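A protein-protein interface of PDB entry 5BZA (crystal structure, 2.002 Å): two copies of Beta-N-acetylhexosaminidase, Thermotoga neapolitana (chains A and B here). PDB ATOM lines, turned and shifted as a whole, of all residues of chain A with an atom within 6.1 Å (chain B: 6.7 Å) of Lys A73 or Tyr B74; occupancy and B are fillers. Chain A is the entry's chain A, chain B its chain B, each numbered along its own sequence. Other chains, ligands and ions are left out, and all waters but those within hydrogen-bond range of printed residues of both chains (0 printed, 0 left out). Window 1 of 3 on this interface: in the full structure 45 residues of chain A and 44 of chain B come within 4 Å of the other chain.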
ATOM      1  N   GLU A  42     -12.526 -15.766  28.073  1.00  0.00           N
ATOM      2  CA  GLU A  42     -12.153 -14.371  27.858  1.00  0.00           C
ATOM      3  C   GLU A  42     -12.384 -13.433  29.066  1.00  0.00           C
ATOM      4  O   GLU A  42     -11.574 -12.505  29.264  1.00  0.00           O
ATOM      5  CB  GLU A  42     -12.852 -13.809  26.641  1.00  0.00           C
ATOM      6  CG  GLU A  42     -12.306 -12.446  26.286  1.00  0.00           C
ATOM      7  CD  GLU A  42     -12.838 -11.957  24.967  1.00  0.00           C
ATOM      8  OE1 GLU A  42     -14.084 -11.774  24.865  1.00  0.00           O
ATOM      9  OE2 GLU A  42     -12.019 -11.742  24.047  1.00  0.00           O
ATOM     10  N   HIS A  64       2.164 -18.578  22.055  1.00  0.00           N
ATOM     11  CA  HIS A  64       1.552 -18.475  20.736  1.00  0.00           C
ATOM     12  C   HIS A  64       2.612 -18.387  19.647  1.00  0.00           C
ATOM     13  O   HIS A  64       3.000 -17.288  19.218  1.00  0.00           O
ATOM     14  CB  HIS A  64       0.586 -17.271  20.656  1.00  0.00           C
ATOM     15  CG  HIS A  64      -0.292 -17.319  19.446  1.00  0.00           C
ATOM     16  ND1 HIS A  64      -1.517 -17.939  19.451  1.00  0.00           N
ATOM     17  CD2 HIS A  64      -0.067 -16.927  18.171  1.00  0.00           C
ATOM     18  CE1 HIS A  64      -2.035 -17.892  18.234  1.00  0.00           C
ATOM     19  NE2 HIS A  64      -1.184 -17.267  17.448  1.00  0.00           N
ATOM     20  N   VAL A  71      -2.590 -20.237  20.864  1.00  0.00           N
ATOM     21  CA  VAL A  71      -3.407 -20.125  22.061  1.00  0.00           C
ATOM     22  C   VAL A  71      -4.235 -18.829  22.139  1.00  0.00           C
ATOM     23  O   VAL A  71      -5.122 -18.727  22.960  1.00  0.00           O
ATOM     24  CB  VAL A  71      -2.552 -20.199  23.316  1.00  0.00           C
ATOM     25  CG1 VAL A  71      -1.995 -21.612  23.493  1.00  0.00           C
ATOM     26  CG2 VAL A  71      -1.459 -19.096  23.294  1.00  0.00           C
ATOM     27  N   LEU A  72      -3.899 -17.863  21.288  1.00  0.00           N
ATOM     28  CA  LEU A  72      -4.548 -16.546  21.215  1.00  0.00           C
ATOM     29  C   LEU A  72      -5.468 -16.494  20.020  1.00  0.00           C
ATOM     30  O   LEU A  72      -5.016 -16.505  18.872  1.00  0.00           O
ATOM     31  CB  LEU A  72      -3.507 -15.434  21.090  1.00  0.00           C
ATOM     32  CG  LEU A  72      -2.533 -15.256  22.263  1.00  0.00           C
ATOM     33  CD1 LEU A  72      -1.500 -14.130  21.974  1.00  0.00           C
ATOM     34  CD2 LEU A  72      -3.290 -15.021  23.572  1.00  0.00           C
ATOM     35  N   LYS A  73      -6.766 -16.413  20.273  1.00  0.00           N
ATOM     36  CA  LYS A  73      -7.708 -16.329  19.168  1.00  0.00           C
ATOM     37  C   LYS A  73      -7.533 -14.995  18.456  1.00  0.00           C
ATOM     38  O   LYS A  73      -7.788 -14.905  17.256  1.00  0.00           O
ATOM     39  CB  LYS A  73      -9.127 -16.498  19.672  1.00  0.00           C
ATOM     40  CG  LYS A  73      -9.684 -15.322  20.430  1.00  0.00           C
ATOM     41  CD  LYS A  73     -11.099 -15.661  20.815  1.00  0.00           C
ATOM     42  CE  LYS A  73     -11.821 -14.586  21.564  1.00  0.00           C
ATOM     43  NZ  LYS A  73     -13.080 -15.267  21.952  1.00  0.00           N
ATOM     44  N   TYR A  74      -6.998 -14.003  19.172  1.00  0.00           N
ATOM     45  CA  TYR A  74      -6.810 -12.655  18.629  1.00  0.00           C
ATOM     46  C   TYR A  74      -5.831 -12.565  17.456  1.00  0.00           C
ATOM     47  O   TYR A  74      -5.910 -11.637  16.684  1.00  0.00           O
ATOM     48  CB  TYR A  74      -6.358 -11.733  19.762  1.00  0.00           C
ATOM     49  CG  TYR A  74      -7.185 -12.006  21.016  1.00  0.00           C
ATOM     50  CD1 TYR A  74      -8.535 -11.604  21.087  1.00  0.00           C
ATOM     51  CD2 TYR A  74      -6.654 -12.720  22.093  1.00  0.00           C
ATOM     52  CE1 TYR A  74      -9.293 -11.887  22.194  1.00  0.00           C
ATOM     53  CE2 TYR A  74      -7.422 -12.983  23.219  1.00  0.00           C
ATOM     54  CZ  TYR A  74      -8.745 -12.563  23.250  1.00  0.00           C
ATOM     55  OH  TYR A  74      -9.531 -12.809  24.348  1.00  0.00           O
ATOM     56  N   VAL A  75      -4.873 -13.499  17.354  1.00  0.00           N
ATOM     57  CA  VAL A  75      -3.920 -13.543  16.243  1.00  0.00           C
ATOM     58  C   VAL A  75      -4.384 -14.484  15.139  1.00  0.00           C
ATOM     59  O   VAL A  75      -4.693 -15.650  15.409  1.00  0.00           O
ATOM     60  CB  VAL A  75      -2.519 -13.980  16.759  1.00  0.00           C
ATOM     61  CG1 VAL A  75      -1.492 -14.027  15.612  1.00  0.00           C
ATOM     62  CG2 VAL A  75      -2.050 -13.018  17.859  1.00  0.00           C
ATOM     63  N   PRO A  76      -4.455 -14.003  13.888  1.00  0.00           N
ATOM     64  CA  PRO A  76      -4.882 -14.953  12.850  1.00  0.00           C
ATOM     65  C   PRO A  76      -3.996 -16.184  12.808  1.00  0.00           C
ATOM     66  O   PRO A  76      -2.772 -16.061  12.936  1.00  0.00           O
ATOM     67  CB  PRO A  76      -4.725 -14.167  11.544  1.00  0.00           C
ATOM     68  CG  PRO A  76      -4.706 -12.784  11.948  1.00  0.00           C
ATOM     69  CD  PRO A  76      -4.196 -12.663  13.339  1.00  0.00           C
ATOM     70  N   SER A  77      -4.629 -17.336  12.596  1.00  0.00           N
ATOM     71  CA  SER A  77      -3.933 -18.608  12.555  1.00  0.00           C
ATOM     72  C   SER A  77      -2.944 -18.629  11.369  1.00  0.00           C
ATOM     73  O   SER A  77      -3.204 -18.050  10.310  1.00  0.00           O
ATOM     74  CB  SER A  77      -4.945 -19.742  12.504  1.00  0.00           C
ATOM     75  OG  SER A  77      -4.264 -20.972  12.611  1.00  0.00           O
ATOM     76  N   ILE A 102      -0.417  -7.246  17.612  1.00  0.00           N
ATOM     77  CA  ILE A 102      -1.630  -7.662  18.273  1.00  0.00           C
ATOM     78  C   ILE A 102      -1.404  -8.028  19.739  1.00  0.00           C
ATOM     79  O   ILE A 102      -2.099  -7.511  20.634  1.00  0.00           O
ATOM     80  CB  ILE A 102      -2.266  -8.827  17.518  1.00  0.00           C
ATOM     81  CG1 ILE A 102      -2.801  -8.297  16.181  1.00  0.00           C
ATOM     82  CG2 ILE A 102      -3.407  -9.384  18.312  1.00  0.00           C
ATOM     83  CD1 ILE A 102      -3.409  -9.313  15.226  1.00  0.00           C
ATOM     84  N   LEU A 106      -2.815  -6.229  23.244  1.00  0.00           N
ATOM     85  CA  LEU A 106      -3.593  -6.893  24.309  1.00  0.00           C
ATOM     86  C   LEU A 106      -3.025  -6.702  25.729  1.00  0.00           C
ATOM     87  O   LEU A 106      -3.797  -6.771  26.719  1.00  0.00           O
ATOM     88  CB  LEU A 106      -3.696  -8.394  24.029  1.00  0.00           C
ATOM     89  CG  LEU A 106      -4.380  -8.878  22.742  1.00  0.00           C
ATOM     90  CD1 LEU A 106      -4.125 -10.378  22.664  1.00  0.00           C
ATOM     91  CD2 LEU A 106      -5.868  -8.545  22.687  1.00  0.00           C
ATOM     92  N   LEU B  39     -15.747 -13.449   7.348  1.00  0.00           N
ATOM     93  CA  LEU B  39     -14.964 -13.392   8.585  1.00  0.00           C
ATOM     94  C   LEU B  39     -15.030 -14.696   9.366  1.00  0.00           C
ATOM     95  O   LEU B  39     -14.063 -15.073  10.033  1.00  0.00           O
ATOM     96  CB  LEU B  39     -15.438 -12.251   9.448  1.00  0.00           C
ATOM     97  CG  LEU B  39     -15.215 -10.901   8.752  1.00  0.00           C
ATOM     98  CD1 LEU B  39     -16.063  -9.815   9.405  1.00  0.00           C
ATOM     99  CD2 LEU B  39     -13.754 -10.498   8.828  1.00  0.00           C
ATOM    100  N   LYS B  41     -14.950 -17.578   8.198  1.00  0.00           N
ATOM    101  CA  LYS B  41     -14.073 -18.546   7.551  1.00  0.00           C
ATOM    102  C   LYS B  41     -12.697 -17.904   7.359  1.00  0.00           C
ATOM    103  O   LYS B  41     -12.421 -17.218   6.363  1.00  0.00           O
ATOM    104  CB  LYS B  41     -14.673 -19.038   6.229  1.00  0.00           C
ATOM    105  CG  LYS B  41     -16.103 -19.717   6.332  1.00  0.00           C
ATOM    106  CD  LYS B  41     -16.554 -20.095   4.912  1.00  0.00           C
ATOM    107  CE  LYS B  41     -17.917 -20.754   4.852  1.00  0.00           C
ATOM    108  NZ  LYS B  41     -18.235 -21.463   6.122  1.00  0.00           N
ATOM    109  N   GLU B  42     -11.848 -18.084   8.368  1.00  0.00           N
ATOM    110  CA  GLU B  42     -10.571 -17.378   8.380  1.00  0.00           C
ATOM    111  C   GLU B  42      -9.769 -17.603   7.109  1.00  0.00           C
ATOM    112  O   GLU B  42      -9.169 -16.657   6.611  1.00  0.00           O
ATOM    113  CB  GLU B  42      -9.758 -17.754   9.599  1.00  0.00           C
ATOM    114  CG  GLU B  42      -8.488 -16.916   9.733  1.00  0.00           C
ATOM    115  CD  GLU B  42      -7.810 -17.148  11.052  1.00  0.00           C
ATOM    116  OE1 GLU B  42      -7.368 -18.300  11.289  1.00  0.00           O
ATOM    117  OE2 GLU B  42      -7.746 -16.187  11.862  1.00  0.00           O
ATOM    118  N   PHE B  45     -11.240 -15.105   4.788  1.00  0.00           N
ATOM    119  CA  PHE B  45     -10.838 -13.755   5.166  1.00  0.00           C
ATOM    120  C   PHE B  45      -9.388 -13.442   4.725  1.00  0.00           C
ATOM    121  O   PHE B  45      -9.137 -12.467   3.995  1.00  0.00           O
ATOM    122  CB  PHE B  45     -11.046 -13.592   6.690  1.00  0.00           C
ATOM    123  CG  PHE B  45     -10.430 -12.344   7.255  1.00  0.00           C
ATOM    124  CD1 PHE B  45     -10.848 -11.088   6.829  1.00  0.00           C
ATOM    125  CD2 PHE B  45      -9.378 -12.429   8.179  1.00  0.00           C
ATOM    126  CE1 PHE B  45     -10.242  -9.913   7.336  1.00  0.00           C
ATOM    127  CE2 PHE B  45      -8.768 -11.274   8.700  1.00  0.00           C
ATOM    128  CZ  PHE B  45      -9.204 -10.012   8.262  1.00  0.00           C
ATOM    129  N   LEU B  46      -8.445 -14.323   5.074  1.00  0.00           N
ATOM    130  CA  LEU B  46      -7.041 -14.119   4.725  1.00  0.00           C
ATOM    131  C   LEU B  46      -6.801 -14.105   3.216  1.00  0.00           C
ATOM    132  O   LEU B  46      -6.040 -13.242   2.704  1.00  0.00           O
ATOM    133  CB  LEU B  46      -6.165 -15.212   5.374  1.00  0.00           C
ATOM    134  CG  LEU B  46      -6.155 -15.212   6.891  1.00  0.00           C
ATOM    135  CD1 LEU B  46      -5.332 -16.392   7.447  1.00  0.00           C
ATOM    136  CD2 LEU B  46      -5.609 -13.882   7.400  1.00  0.00           C
ATOM    137  N   HIS B  64     -17.659  -3.898  13.250  1.00  0.00           N
ATOM    138  CA  HIS B  64     -17.282  -4.314  14.574  1.00  0.00           C
ATOM    139  C   HIS B  64     -17.392  -3.167  15.560  1.00  0.00           C
ATOM    140  O   HIS B  64     -16.427  -2.458  15.812  1.00  0.00           O
ATOM    141  CB  HIS B  64     -15.861  -4.926  14.603  1.00  0.00           C
ATOM    142  CG  HIS B  64     -15.555  -5.610  15.900  1.00  0.00           C
ATOM    143  ND1 HIS B  64     -15.791  -6.950  16.107  1.00  0.00           N
ATOM    144  CD2 HIS B  64     -15.146  -5.111  17.090  1.00  0.00           C
ATOM    145  CE1 HIS B  64     -15.488  -7.256  17.357  1.00  0.00           C
ATOM    146  NE2 HIS B  64     -15.103  -6.157  17.979  1.00  0.00           N
ATOM    147  N   VAL B  71     -17.939  -8.736  15.123  1.00  0.00           N
ATOM    148  CA  VAL B  71     -17.768  -9.665  14.012  1.00  0.00           C
ATOM    149  C   VAL B  71     -16.307 -10.130  13.879  1.00  0.00           C
ATOM    150  O   VAL B  71     -16.029 -11.097  13.192  1.00  0.00           O
ATOM    151  CB  VAL B  71     -18.212  -9.040  12.726  1.00  0.00           C
ATOM    152  CG1 VAL B  71     -19.729  -8.756  12.800  1.00  0.00           C
ATOM    153  CG2 VAL B  71     -17.414  -7.774  12.474  1.00  0.00           C
ATOM    154  N   LEU B  72     -15.400  -9.445  14.567  1.00  0.00           N
ATOM    155  CA  LEU B  72     -13.983  -9.757  14.514  1.00  0.00           C
ATOM    156  C   LEU B  72     -13.574 -10.529  15.766  1.00  0.00           C
ATOM    157  O   LEU B  72     -13.556  -9.988  16.874  1.00  0.00           O
ATOM    158  CB  LEU B  72     -13.149  -8.485  14.387  1.00  0.00           C
ATOM    159  CG  LEU B  72     -13.316  -7.617  13.139  1.00  0.00           C
ATOM    160  CD1 LEU B  72     -12.385  -6.390  13.154  1.00  0.00           C
ATOM    161  CD2 LEU B  72     -13.115  -8.468  11.877  1.00  0.00           C
ATOM    162  N   LYS B  73     -13.203 -11.801  15.587  1.00  0.00           N
ATOM    163  CA  LYS B  73     -12.809 -12.574  16.751  1.00  0.00           C
ATOM    164  C   LYS B  73     -11.482 -12.058  17.309  1.00  0.00           C
ATOM    165  O   LYS B  73     -11.143 -12.341  18.460  1.00  0.00           O
ATOM    166  CB  LYS B  73     -12.688 -14.041  16.422  1.00  0.00           C
ATOM    167  CG  LYS B  73     -11.456 -14.396  15.634  1.00  0.00           C
ATOM    168  CD  LYS B  73     -11.394 -15.887  15.545  1.00  0.00           C
ATOM    169  CE  LYS B  73     -10.148 -16.365  14.875  1.00  0.00           C
ATOM    170  NZ  LYS B  73     -10.282 -17.835  14.834  1.00  0.00           N
ATOM    171  N   TYR B  74     -10.739 -11.340  16.463  1.00  0.00           N
ATOM    172  CA  TYR B  74      -9.439 -10.759  16.810  1.00  0.00           C
ATOM    173  C   TYR B  74      -9.489  -9.659  17.859  1.00  0.00           C
ATOM    174  O   TYR B  74      -8.533  -9.490  18.633  1.00  0.00           O
ATOM    175  CB  TYR B  74      -8.810 -10.224  15.538  1.00  0.00           C
ATOM    176  CG  TYR B  74      -8.939 -11.239  14.408  1.00  0.00           C
ATOM    177  CD1 TYR B  74      -8.154 -12.427  14.410  1.00  0.00           C
ATOM    178  CD2 TYR B  74      -9.856 -11.043  13.360  1.00  0.00           C
ATOM    179  CE1 TYR B  74      -8.289 -13.359  13.404  1.00  0.00           C
ATOM    180  CE2 TYR B  74      -9.971 -11.967  12.328  1.00  0.00           C
ATOM    181  CZ  TYR B  74      -9.193 -13.126  12.365  1.00  0.00           C
ATOM    182  OH  TYR B  74      -9.317 -14.049  11.361  1.00  0.00           O
ATOM    183  N   VAL B  75     -10.614  -8.924  17.895  1.00  0.00           N
ATOM    184  CA  VAL B  75     -10.824  -7.899  18.893  1.00  0.00           C
ATOM    185  C   VAL B  75     -11.490  -8.496  20.110  1.00  0.00           C
ATOM    186  O   VAL B  75     -12.532  -9.137  19.997  1.00  0.00           O
ATOM    187  CB  VAL B  75     -11.730  -6.742  18.358  1.00  0.00           C
ATOM    188  CG1 VAL B  75     -11.907  -5.667  19.441  1.00  0.00           C
ATOM    189  CG2 VAL B  75     -11.110  -6.131  17.137  1.00  0.00           C
ATOM    190  N   PRO B  76     -10.883  -8.322  21.281  1.00  0.00           N
ATOM    191  CA  PRO B  76     -11.586  -8.847  22.466  1.00  0.00           C
ATOM    192  C   PRO B  76     -12.943  -8.184  22.649  1.00  0.00           C
ATOM    193  O   PRO B  76     -13.111  -6.992  22.389  1.00  0.00           O
ATOM    194  CB  PRO B  76     -10.664  -8.530  23.653  1.00  0.00           C
ATOM    195  CG  PRO B  76      -9.485  -7.757  23.090  1.00  0.00           C
ATOM    196  CD  PRO B  76      -9.557  -7.754  21.568  1.00  0.00           C
ATOM    197  N   SER B  77     -13.893  -8.986  23.104  1.00  0.00           N
ATOM    198  CA  SER B  77     -15.255  -8.554  23.339  1.00  0.00           C
ATOM    199  C   SER B  77     -15.421  -7.442  24.408  1.00  0.00           C
ATOM    200  O   SER B  77     -14.768  -7.414  25.465  1.00  0.00           O
ATOM    201  CB  SER B  77     -16.093  -9.776  23.719  1.00  0.00           C
ATOM    202  OG  SER B  77     -17.433  -9.385  23.890  1.00  0.00           O
ATOM    203  N   MET B  98      -7.477   0.360  21.113  1.00  0.00           N
ATOM    204  CA  MET B  98      -7.109  -1.048  21.152  1.00  0.00           C
ATOM    205  C   MET B  98      -7.688  -1.743  19.913  1.00  0.00           C
ATOM    206  O   MET B  98      -6.967  -2.415  19.140  1.00  0.00           O
ATOM    207  CB  MET B  98      -7.650  -1.673  22.438  1.00  0.00           C
ATOM    208  CG  MET B  98      -7.290  -3.143  22.672  1.00  0.00           C
ATOM    209  SD  MET B  98      -8.527  -4.070  23.626  1.00  0.00           S
ATOM    210  CE  MET B  98      -9.757  -4.279  22.354  1.00  0.00           C
ATOM    211  N   ILE B 102      -5.694  -3.235  16.550  1.00  0.00           N
ATOM    212  CA  ILE B 102      -5.866  -4.594  16.071  1.00  0.00           C
ATOM    213  C   ILE B 102      -6.407  -4.665  14.626  1.00  0.00           C
ATOM    214  O   ILE B 102      -5.818  -5.370  13.780  1.00  0.00           O
ATOM    215  CB  ILE B 102      -6.771  -5.378  17.038  1.00  0.00           C
ATOM    216  CG1 ILE B 102      -6.058  -5.562  18.381  1.00  0.00           C
ATOM    217  CG2 ILE B 102      -7.074  -6.703  16.464  1.00  0.00           C
ATOM    218  CD1 ILE B 102      -6.874  -6.259  19.459  1.00  0.00           C
ATOM    219  N   MET B 103      -7.477  -3.894  14.326  1.00  0.00           N
ATOM    220  CA  MET B 103      -8.099  -3.839  13.003  1.00  0.00           C
ATOM    221  C   MET B 103      -7.103  -3.410  11.935  1.00  0.00           C
ATOM    222  O   MET B 103      -7.002  -4.024  10.848  1.00  0.00           O
ATOM    223  CB  MET B 103      -9.290  -2.839  12.991  1.00  0.00           C
ATOM    224  CG  MET B 103     -10.511  -3.255  13.768  1.00  0.00           C
ATOM    225  SD  MET B 103     -11.752  -1.927  14.104  1.00  0.00           S
ATOM    226  CE  MET B 103     -12.798  -2.820  15.267  1.00  0.00           C
ATOM    227  N   LEU B 106      -4.720  -6.014  11.081  1.00  0.00           N
ATOM    228  CA  LEU B 106      -5.248  -7.059  10.208  1.00  0.00           C
ATOM    229  C   LEU B 106      -5.315  -6.661   8.751  1.00  0.00           C
ATOM    230  O   LEU B 106      -5.264  -7.526   7.874  1.00  0.00           O
ATOM    231  CB  LEU B 106      -6.622  -7.507  10.664  1.00  0.00           C
ATOM    232  CG  LEU B 106      -6.739  -8.217  12.007  1.00  0.00           C
ATOM    233  CD1 LEU B 106      -8.246  -8.315  12.330  1.00  0.00           C
ATOM    234  CD2 LEU B 106      -6.074  -9.608  11.916  1.00  0.00           C
ATOM    235  N   PHE B 108      -7.683  -3.792   8.059  1.00  0.00           N
ATOM    236  CA  PHE B 108      -8.833  -2.860   7.955  1.00  0.00           C
ATOM    237  C   PHE B 108      -8.319  -1.394   7.980  1.00  0.00           C
ATOM    238  O   PHE B 108      -7.212  -1.144   8.441  1.00  0.00           O
ATOM    239  CB  PHE B 108      -9.847  -3.125   9.080  1.00  0.00           C
ATOM    240  CG  PHE B 108     -10.594  -4.430   8.927  1.00  0.00           C
ATOM    241  CD1 PHE B 108     -11.776  -4.499   8.179  1.00  0.00           C
ATOM    242  CD2 PHE B 108     -10.061  -5.621   9.472  1.00  0.00           C
ATOM    243  CE1 PHE B 108     -12.466  -5.721   8.025  1.00  0.00           C
ATOM    244  CE2 PHE B 108     -10.716  -6.854   9.318  1.00  0.00           C
ATOM    245  CZ  PHE B 108     -11.921  -6.907   8.591  1.00  0.00           C
ATOM    246  N   SER B 322      -2.906  -8.822   6.813  1.00  0.00           N
ATOM    247  CA  SER B 322      -2.858 -10.212   7.266  1.00  0.00           C
ATOM    248  C   SER B 322      -2.957 -11.232   6.096  1.00  0.00           C
ATOM    249  O   SER B 322      -2.790 -12.440   6.286  1.00  0.00           O
ATOM    250  CB  SER B 322      -3.930 -10.449   8.338  1.00  0.00           C
ATOM    251  OG  SER B 322      -5.270 -10.269   7.859  1.00  0.00           O
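N of Ser B77 lies close to OE1 of Glu A42, 3.3 Å away.
N of Ser A77 sits close to OE1 of Glu B42.
The side-chain carboxylate of Glu A42 sits at hydrogen-bond distance from the side-chain hydroxyl of Tyr A74 (2.7 Å).
The side-chain hydroxyl (OH) of Tyr B74 lies within hydrogen-bond range of the side-chain carboxylate (OE2) of Glu B42 (2.7 Å).
The backbone carbonyl oxygen (O) of Leu B106 sits at hydrogen-bond distance from the side-chain hydroxyl (OG) of Ser B322, at 2.7 Å.
OE2 of Glu A42 touches CA of Pro B76, 3.3 Å away.
O of Lys A73 touches CE of Lys B73, at 3.7 Å.
O of Lys A73 touches CD1 of Tyr B74, at 3.8 Å.
Lys B73 touches Tyr A74.
Tyr A74 touches Tyr B74 (CD1 to O, 3.2 Å).
Tyr A74 touches Pro B76 (CE1 to CA, 3.8 Å).
Pro A76 touches Glu B42 (CA to OE2, 3.3 Å).
CA of Pro A76 touches CE1 of Tyr B74, 3.8 Å away.
Leu B106 touches Pro A76 (CD2 to CG, 3.5 Å).
Leu A106 touches Pro B76.
Lys A73 touches two residues of chain B.
Tyr B74 touches just these residues of chain A: Lys A73, Tyr A74 and Pro A76.
Printed residues of chain A within 4 Å of Glu B42: Pro A76 (3.3 Å) and Ser A77 (3.1 Å).
Printed residues of chain B within 4 Å of Tyr A74: Lys B73, Tyr B74 and Pro B76.
Printed residues of chain A within 4 Å of Lys B73: Lys A73 and Tyr A74.
Of the printed residues of chain A, Leu B46 touches Ser A77.
Printed residues of chain B within 4 Å of Ser A77: Glu B42 and Leu B46.
Val B71 touches none of the printed residues of chain A.
The nearest residue of chain B that does not touch Lys A73 is Glu B42 (5.5 Å).
Of the 19 printed residues of chain B, 7 touch a printed residue of chain A.
Along chain B the printed residues that touch a printed residue of chain A span positions 42 to 106.
Hydrophobic or aromatic side chains of chain A within 4 Å of the printed part of chain B: Tyr A74, Pro A76 and Leu A106.
Among the printed residues, 13 pairs touch across the chains.
Lys A73 touches its own counterpart, Lys B73.
Lys A73 touches Tyr B74, and with the chains exchanged Tyr A74 touches Lys B73.
Tyr B74 touches its own counterpart, Tyr A74.
Pro A76 touches Leu B106, and with the chains exchanged Leu A106 touches Pro B76.
Positions printed for both chains: 42, 64, 71, 72, 73, 74, 75, 76, 77, 102 and 106.
Of the 13 pairs that touch across the chains among the printed residues, 12 have their exchanged pair printed and touching as well.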
